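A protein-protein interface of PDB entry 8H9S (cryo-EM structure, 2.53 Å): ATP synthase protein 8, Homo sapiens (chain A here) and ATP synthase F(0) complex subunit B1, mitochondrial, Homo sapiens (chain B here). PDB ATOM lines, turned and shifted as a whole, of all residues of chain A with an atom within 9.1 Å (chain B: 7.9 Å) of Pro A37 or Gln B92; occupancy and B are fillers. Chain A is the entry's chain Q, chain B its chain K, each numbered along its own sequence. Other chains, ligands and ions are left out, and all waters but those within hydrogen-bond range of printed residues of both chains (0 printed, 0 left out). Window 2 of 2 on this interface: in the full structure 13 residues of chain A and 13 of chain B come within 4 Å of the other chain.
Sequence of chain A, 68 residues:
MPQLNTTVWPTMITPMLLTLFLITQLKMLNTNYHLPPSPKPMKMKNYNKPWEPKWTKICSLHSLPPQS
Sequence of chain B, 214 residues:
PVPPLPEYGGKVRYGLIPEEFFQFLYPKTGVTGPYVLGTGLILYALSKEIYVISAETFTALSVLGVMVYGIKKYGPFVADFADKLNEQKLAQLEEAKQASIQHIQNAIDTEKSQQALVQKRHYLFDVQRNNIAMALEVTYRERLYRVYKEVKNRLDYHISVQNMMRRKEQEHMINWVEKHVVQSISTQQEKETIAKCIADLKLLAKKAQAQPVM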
ATOM      1  N   HIS A  34       4.930  -0.449 -19.196  1.00  0.00           N
ATOM      2  CA  HIS A  34       4.214   0.675 -18.621  1.00  0.00           C
ATOM      3  C   HIS A  34       2.718   0.535 -18.875  1.00  0.00           C
ATOM      4  O   HIS A  34       2.273  -0.205 -19.753  1.00  0.00           O
ATOM      5  CB  HIS A  34       4.728   1.989 -19.198  1.00  0.00           C
ATOM      6  CG  HIS A  34       4.420   2.173 -20.649  1.00  0.00           C
ATOM      7  ND1 HIS A  34       3.171   2.530 -21.106  1.00  0.00           N
ATOM      8  CD2 HIS A  34       5.197   2.042 -21.748  1.00  0.00           C
ATOM      9  CE1 HIS A  34       3.192   2.613 -22.422  1.00  0.00           C
ATOM     10  NE2 HIS A  34       4.411   2.322 -22.836  1.00  0.00           N
ATOM     11  N   LEU A  35       1.924   1.200 -18.026  1.00  0.00           N
ATOM     12  CA  LEU A  35       0.449   1.137 -18.114  1.00  0.00           C
ATOM     13  C   LEU A  35       0.034   1.997 -19.295  1.00  0.00           C
ATOM     14  O   LEU A  35       0.790   2.879 -19.647  1.00  0.00           O
ATOM     15  CB  LEU A  35      -0.109   1.616 -16.783  1.00  0.00           C
ATOM     16  CG  LEU A  35      -0.163   0.578 -15.667  1.00  0.00           C
ATOM     17  CD1 LEU A  35       1.229   0.143 -15.265  1.00  0.00           C
ATOM     18  CD2 LEU A  35      -0.896   1.137 -14.464  1.00  0.00           C
ATOM     19  N   PRO A  36      -1.117   1.738 -19.962  1.00  0.00           N
ATOM     20  CA  PRO A  36      -1.489   2.472 -21.183  1.00  0.00           C
ATOM     21  C   PRO A  36      -1.568   3.996 -21.022  1.00  0.00           C
ATOM     22  O   PRO A  36      -1.985   4.453 -19.973  1.00  0.00           O
ATOM     23  CB  PRO A  36      -2.897   1.947 -21.506  1.00  0.00           C
ATOM     24  CG  PRO A  36      -2.931   0.576 -20.875  1.00  0.00           C
ATOM     25  CD  PRO A  36      -2.125   0.731 -19.604  1.00  0.00           C
ATOM     26  N   PRO A  37      -1.175   4.788 -22.044  1.00  0.00           N
ATOM     27  CA  PRO A  37      -1.315   6.244 -21.986  1.00  0.00           C
ATOM     28  C   PRO A  37      -2.783   6.607 -22.244  1.00  0.00           C
ATOM     29  O   PRO A  37      -3.094   7.041 -23.332  1.00  0.00           O
ATOM     30  CB  PRO A  37      -0.421   6.724 -23.137  1.00  0.00           C
ATOM     31  CG  PRO A  37      -0.475   5.590 -24.137  1.00  0.00           C
ATOM     32  CD  PRO A  37      -0.575   4.330 -23.300  1.00  0.00           C
ATOM     33  N   SER A  38      -3.647   6.393 -21.251  1.00  0.00           N
ATOM     34  CA  SER A  38      -5.102   6.670 -21.412  1.00  0.00           C
ATOM     35  C   SER A  38      -5.389   8.101 -20.981  1.00  0.00           C
ATOM     36  O   SER A  38      -5.357   8.371 -19.780  1.00  0.00           O
ATOM     37  CB  SER A  38      -5.930   5.712 -20.617  1.00  0.00           C
ATOM     38  OG  SER A  38      -6.008   6.115 -19.259  1.00  0.00           O
ATOM     39  N   PRO A  39      -5.672   9.021 -21.911  1.00  0.00           N
ATOM     40  CA  PRO A  39      -5.840  10.431 -21.558  1.00  0.00           C
ATOM     41  C   PRO A  39      -7.298  10.850 -21.329  1.00  0.00           C
ATOM     42  O   PRO A  39      -8.061  10.864 -22.271  1.00  0.00           O
ATOM     43  CB  PRO A  39      -5.263  11.094 -22.807  1.00  0.00           C
ATOM     44  CG  PRO A  39      -5.630  10.153 -23.941  1.00  0.00           C
ATOM     45  CD  PRO A  39      -5.802   8.773 -23.340  1.00  0.00           C
ATOM     46  N   LYS A  40      -7.651  11.160 -20.078  1.00  0.00           N
ATOM     47  CA  LYS A  40      -9.062  11.502 -19.752  1.00  0.00           C
ATOM     48  C   LYS A  40      -9.358  12.946 -20.170  1.00  0.00           C
ATOM     49  O   LYS A  40      -8.836  13.873 -19.518  1.00  0.00           O
ATOM     50  CB  LYS A  40      -9.340  11.275 -18.262  1.00  0.00           C
ATOM     51  CG  LYS A  40      -9.299   9.826 -17.795  1.00  0.00           C
ATOM     52  CD  LYS A  40      -9.556   9.657 -16.311  1.00  0.00           C
ATOM     53  CE  LYS A  40      -9.540   8.215 -15.847  1.00  0.00           C
ATOM     54  NZ  LYS A  40      -9.771   8.089 -14.389  1.00  0.00           N
ATOM     55  N   LEU B  85       4.325  -3.654 -34.460  1.00  0.00           N
ATOM     56  CA  LEU B  85       4.221  -3.428 -33.023  1.00  0.00           C
ATOM     57  C   LEU B  85       4.685  -2.024 -32.668  1.00  0.00           C
ATOM     58  O   LEU B  85       4.010  -1.294 -31.925  1.00  0.00           O
ATOM     59  CB  LEU B  85       5.048  -4.463 -32.268  1.00  0.00           C
ATOM     60  CG  LEU B  85       4.384  -5.782 -31.893  1.00  0.00           C
ATOM     61  CD1 LEU B  85       5.285  -6.557 -30.966  1.00  0.00           C
ATOM     62  CD2 LEU B  85       3.053  -5.524 -31.241  1.00  0.00           C
ATOM     63  N   ASN B  86       5.831  -1.616 -33.213  1.00  0.00           N
ATOM     64  CA  ASN B  86       6.345  -0.288 -32.899  1.00  0.00           C
ATOM     65  C   ASN B  86       5.446   0.804 -33.465  1.00  0.00           C
ATOM     66  O   ASN B  86       5.220   1.828 -32.810  1.00  0.00           O
ATOM     67  CB  ASN B  86       7.767  -0.140 -33.424  1.00  0.00           C
ATOM     68  CG  ASN B  86       8.789  -0.710 -32.476  1.00  0.00           C
ATOM     69  OD1 ASN B  86       8.583  -0.729 -31.265  1.00  0.00           O
ATOM     70  ND2 ASN B  86       9.901  -1.183 -33.021  1.00  0.00           N
ATOM     71  N   GLU B  87       4.912   0.601 -34.671  1.00  0.00           N
ATOM     72  CA  GLU B  87       4.041   1.606 -35.271  1.00  0.00           C
ATOM     73  C   GLU B  87       2.739   1.745 -34.500  1.00  0.00           C
ATOM     74  O   GLU B  87       2.233   2.858 -34.333  1.00  0.00           O
ATOM     75  CB  GLU B  87       3.763   1.259 -36.730  1.00  0.00           C
ATOM     76  CG  GLU B  87       4.779   1.838 -37.689  1.00  0.00           C
ATOM     77  CD  GLU B  87       4.407   1.619 -39.139  1.00  0.00           C
ATOM     78  OE1 GLU B  87       3.343   2.115 -39.561  1.00  0.00           O
ATOM     79  OE2 GLU B  87       5.182   0.954 -39.858  1.00  0.00           O
ATOM     80  N   GLN B  88       2.185   0.636 -34.014  1.00  0.00           N
ATOM     81  CA  GLN B  88       0.974   0.719 -33.210  1.00  0.00           C
ATOM     82  C   GLN B  88       1.235   1.426 -31.890  1.00  0.00           C
ATOM     83  O   GLN B  88       0.414   2.235 -31.445  1.00  0.00           O
ATOM     84  CB  GLN B  88       0.402  -0.673 -32.964  1.00  0.00           C
ATOM     85  CG  GLN B  88      -0.189  -1.327 -34.193  1.00  0.00           C
ATOM     86  CD  GLN B  88      -0.573  -2.769 -33.946  1.00  0.00           C
ATOM     87  OE1 GLN B  88      -0.946  -3.491 -34.869  1.00  0.00           O
ATOM     88  NE2 GLN B  88      -0.482  -3.198 -32.693  1.00  0.00           N
ATOM     89  N   LYS B  89       2.372   1.147 -31.250  1.00  0.00           N
ATOM     90  CA  LYS B  89       2.672   1.853 -30.008  1.00  0.00           C
ATOM     91  C   LYS B  89       2.847   3.346 -30.250  1.00  0.00           C
ATOM     92  O   LYS B  89       2.345   4.172 -29.478  1.00  0.00           O
ATOM     93  CB  LYS B  89       3.920   1.275 -29.352  1.00  0.00           C
ATOM     94  CG  LYS B  89       4.090   1.694 -27.910  1.00  0.00           C
ATOM     95  CD  LYS B  89       5.240   0.958 -27.271  1.00  0.00           C
ATOM     96  CE  LYS B  89       5.438   1.393 -25.840  1.00  0.00           C
ATOM     97  NZ  LYS B  89       6.528   0.615 -25.196  1.00  0.00           N
ATOM     98  N   LEU B  90       3.540   3.713 -31.328  1.00  0.00           N
ATOM     99  CA  LEU B  90       3.744   5.124 -31.633  1.00  0.00           C
ATOM    100  C   LEU B  90       2.427   5.821 -31.948  1.00  0.00           C
ATOM    101  O   LEU B  90       2.188   6.950 -31.498  1.00  0.00           O
ATOM    102  CB  LEU B  90       4.719   5.261 -32.798  1.00  0.00           C
ATOM    103  CG  LEU B  90       5.192   6.661 -33.159  1.00  0.00           C
ATOM    104  CD1 LEU B  90       6.249   7.133 -32.192  1.00  0.00           C
ATOM    105  CD2 LEU B  90       5.720   6.673 -34.578  1.00  0.00           C
ATOM    106  N   ALA B  91       1.560   5.167 -32.724  1.00  0.00           N
ATOM    107  CA  ALA B  91       0.265   5.752 -33.047  1.00  0.00           C
ATOM    108  C   ALA B  91      -0.584   5.938 -31.800  1.00  0.00           C
ATOM    109  O   ALA B  91      -1.214   6.987 -31.622  1.00  0.00           O
ATOM    110  CB  ALA B  91      -0.462   4.876 -34.063  1.00  0.00           C
ATOM    111  N   GLN B  92      -0.620   4.931 -30.927  1.00  0.00           N
ATOM    112  CA  GLN B  92      -1.372   5.062 -29.687  1.00  0.00           C
ATOM    113  C   GLN B  92      -0.835   6.199 -28.831  1.00  0.00           C
ATOM    114  O   GLN B  92      -1.607   6.945 -28.220  1.00  0.00           O
ATOM    115  CB  GLN B  92      -1.334   3.750 -28.915  1.00  0.00           C
ATOM    116  CG  GLN B  92      -2.000   3.816 -27.567  1.00  0.00           C
ATOM    117  CD  GLN B  92      -2.069   2.468 -26.897  1.00  0.00           C
ATOM    118  OE1 GLN B  92      -1.612   1.468 -27.445  1.00  0.00           O
ATOM    119  NE2 GLN B  92      -2.645   2.428 -25.704  1.00  0.00           N
ATOM    120  N   LEU B  93       0.486   6.366 -28.791  1.00  0.00           N
ATOM    121  CA  LEU B  93       1.053   7.433 -27.974  1.00  0.00           C
ATOM    122  C   LEU B  93       0.712   8.807 -28.536  1.00  0.00           C
ATOM    123  O   LEU B  93       0.346   9.718 -27.783  1.00  0.00           O
ATOM    124  CB  LEU B  93       2.565   7.257 -27.861  1.00  0.00           C
ATOM    125  CG  LEU B  93       3.062   6.142 -26.942  1.00  0.00           C
ATOM    126  CD1 LEU B  93       4.559   5.985 -27.080  1.00  0.00           C
ATOM    127  CD2 LEU B  93       2.687   6.422 -25.505  1.00  0.00           C
ATOM    128  N   GLU B  94       0.825   8.981 -29.855  1.00  0.00           N
ATOM    129  CA  GLU B  94       0.486  10.271 -30.450  1.00  0.00           C
ATOM    130  C   GLU B  94      -0.990  10.593 -30.257  1.00  0.00           C
ATOM    131  O   GLU B  94      -1.356  11.740 -29.957  1.00  0.00           O
ATOM    132  CB  GLU B  94       0.854  10.278 -31.930  1.00  0.00           C
ATOM    133  CG  GLU B  94       2.350  10.322 -32.177  1.00  0.00           C
ATOM    134  CD  GLU B  94       2.716  10.158 -33.638  1.00  0.00           C
ATOM    135  OE1 GLU B  94       1.865   9.688 -34.421  1.00  0.00           O
ATOM    136  OE2 GLU B  94       3.861  10.496 -34.003  1.00  0.00           O
ATOM    137  N   GLU B  95      -1.853   9.590 -30.424  1.00  0.00           N
ATOM    138  CA  GLU B  95      -3.274   9.770 -30.154  1.00  0.00           C
ATOM    139  C   GLU B  95      -3.509  10.220 -28.718  1.00  0.00           C
ATOM    140  O   GLU B  95      -4.261  11.169 -28.469  1.00  0.00           O
ATOM    141  CB  GLU B  95      -4.018   8.469 -30.449  1.00  0.00           C
ATOM    142  CG  GLU B  95      -5.503   8.511 -30.170  1.00  0.00           C
ATOM    143  CD  GLU B  95      -5.839   8.050 -28.767  1.00  0.00           C
ATOM    144  OE1 GLU B  95      -5.091   7.211 -28.228  1.00  0.00           O
ATOM    145  OE2 GLU B  95      -6.843   8.529 -28.202  1.00  0.00           O
ATOM    146  N   ALA B  96      -2.871   9.553 -27.756  1.00  0.00           N
ATOM    147  CA  ALA B  96      -3.102   9.896 -26.359  1.00  0.00           C
ATOM    148  C   ALA B  96      -2.493  11.234 -25.979  1.00  0.00           C
ATOM    149  O   ALA B  96      -2.898  11.820 -24.974  1.00  0.00           O
ATOM    150  CB  ALA B  96      -2.552   8.802 -25.453  1.00  0.00           C
ATOM    151  N   LYS B  97      -1.528  11.731 -26.747  1.00  0.00           N
ATOM    152  CA  LYS B  97      -1.019  13.074 -26.486  1.00  0.00           C
ATOM    153  C   LYS B  97      -1.986  14.133 -27.004  1.00  0.00           C
ATOM    154  O   LYS B  97      -2.341  15.079 -26.281  1.00  0.00           O
ATOM    155  CB  LYS B  97       0.357  13.239 -27.121  1.00  0.00           C
ATOM    156  CG  LYS B  97       0.829  14.661 -27.249  1.00  0.00           C
ATOM    157  CD  LYS B  97       1.947  14.735 -28.261  1.00  0.00           C
ATOM    158  CE  LYS B  97       2.622  16.082 -28.262  1.00  0.00           C
ATOM    159  NZ  LYS B  97       3.951  15.994 -28.913  1.00  0.00           N
ATOM    160  N   GLN B  98      -2.421  13.982 -28.259  1.00  0.00           N
ATOM    161  CA  GLN B  98      -3.421  14.895 -28.800  1.00  0.00           C
ATOM    162  C   GLN B  98      -4.688  14.907 -27.956  1.00  0.00           C
ATOM    163  O   GLN B  98      -5.338  15.950 -27.829  1.00  0.00           O
ATOM    164  CB  GLN B  98      -3.750  14.517 -30.240  1.00  0.00           C
ATOM    165  CG  GLN B  98      -2.569  14.607 -31.180  1.00  0.00           C
ATOM    166  CD  GLN B  98      -2.026  16.012 -31.292  1.00  0.00           C
ATOM    167  OE1 GLN B  98      -0.814  16.227 -31.279  1.00  0.00           O
ATOM    168  NE2 GLN B  98      -2.923  16.983 -31.406  1.00  0.00           N
ATOM    169  N   ALA B  99      -5.051  13.768 -27.363  1.00  0.00           N
ATOM    170  CA  ALA B  99      -6.261  13.721 -26.550  1.00  0.00           C
ATOM    171  C   ALA B  99      -6.155  14.632 -25.335  1.00  0.00           C
ATOM    172  O   ALA B  99      -7.105  15.348 -25.003  1.00  0.00           O
ATOM    173  CB  ALA B  99      -6.549  12.287 -26.118  1.00  0.00           C
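Of the 7 printed residues of chain A, 3 touch a printed residue of chain B.
Hydrophobic or aromatic side chains of chain A within 4 Å of the printed part of chain B: His A34, Pro A37 and Pro A39.
Hydrophobic or aromatic side chains of chain B that line the printed part of chain A: Leu B93, Ala B96 and Ala B99.
Among the printed residues, no Asp or Glu carboxylate lies within 4 Å of a Lys or Arg side-chain nitrogen of the other chain.
Among the printed residues, pairs that only touch across the chains: His A34 with Lys B89 (3.3 Å), Pro A37 with Gln B92 (3.7 Å), Pro A37 with Leu B93 (3.5 Å), Pro A37 with Ala B96 (2.8 Å), Pro A39 with Ala B96 (3.3 Å) and Pro A39 with Ala B99 (3.2 Å).
Of chain B, only Gln B92 (3.7 Å), Leu B93 (3.5 Å) and Ala B96 (2.8 Å) come within 4 Å of Pro A37.
Gln B92 touches just one residue of chain A: Pro A37.
Of the printed residues of chain A, Ala B99 touches Pro A39.
Of the printed residues of chain A, Leu B93 touches Pro A37.
Of the printed residues of chain B, His A34 touches Lys B89 (3.3 Å).
Of the printed residues of chain A, Lys B89 touches His A34.
Asn B86 touches none of the printed residues of chain A.
The nearest residue of chain B that does not touch Pro A37 is Glu B95 (5.3 Å).
The nearest printed residue of chain A that does not touch Lys B89 is Pro A37 (6.2 Å).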
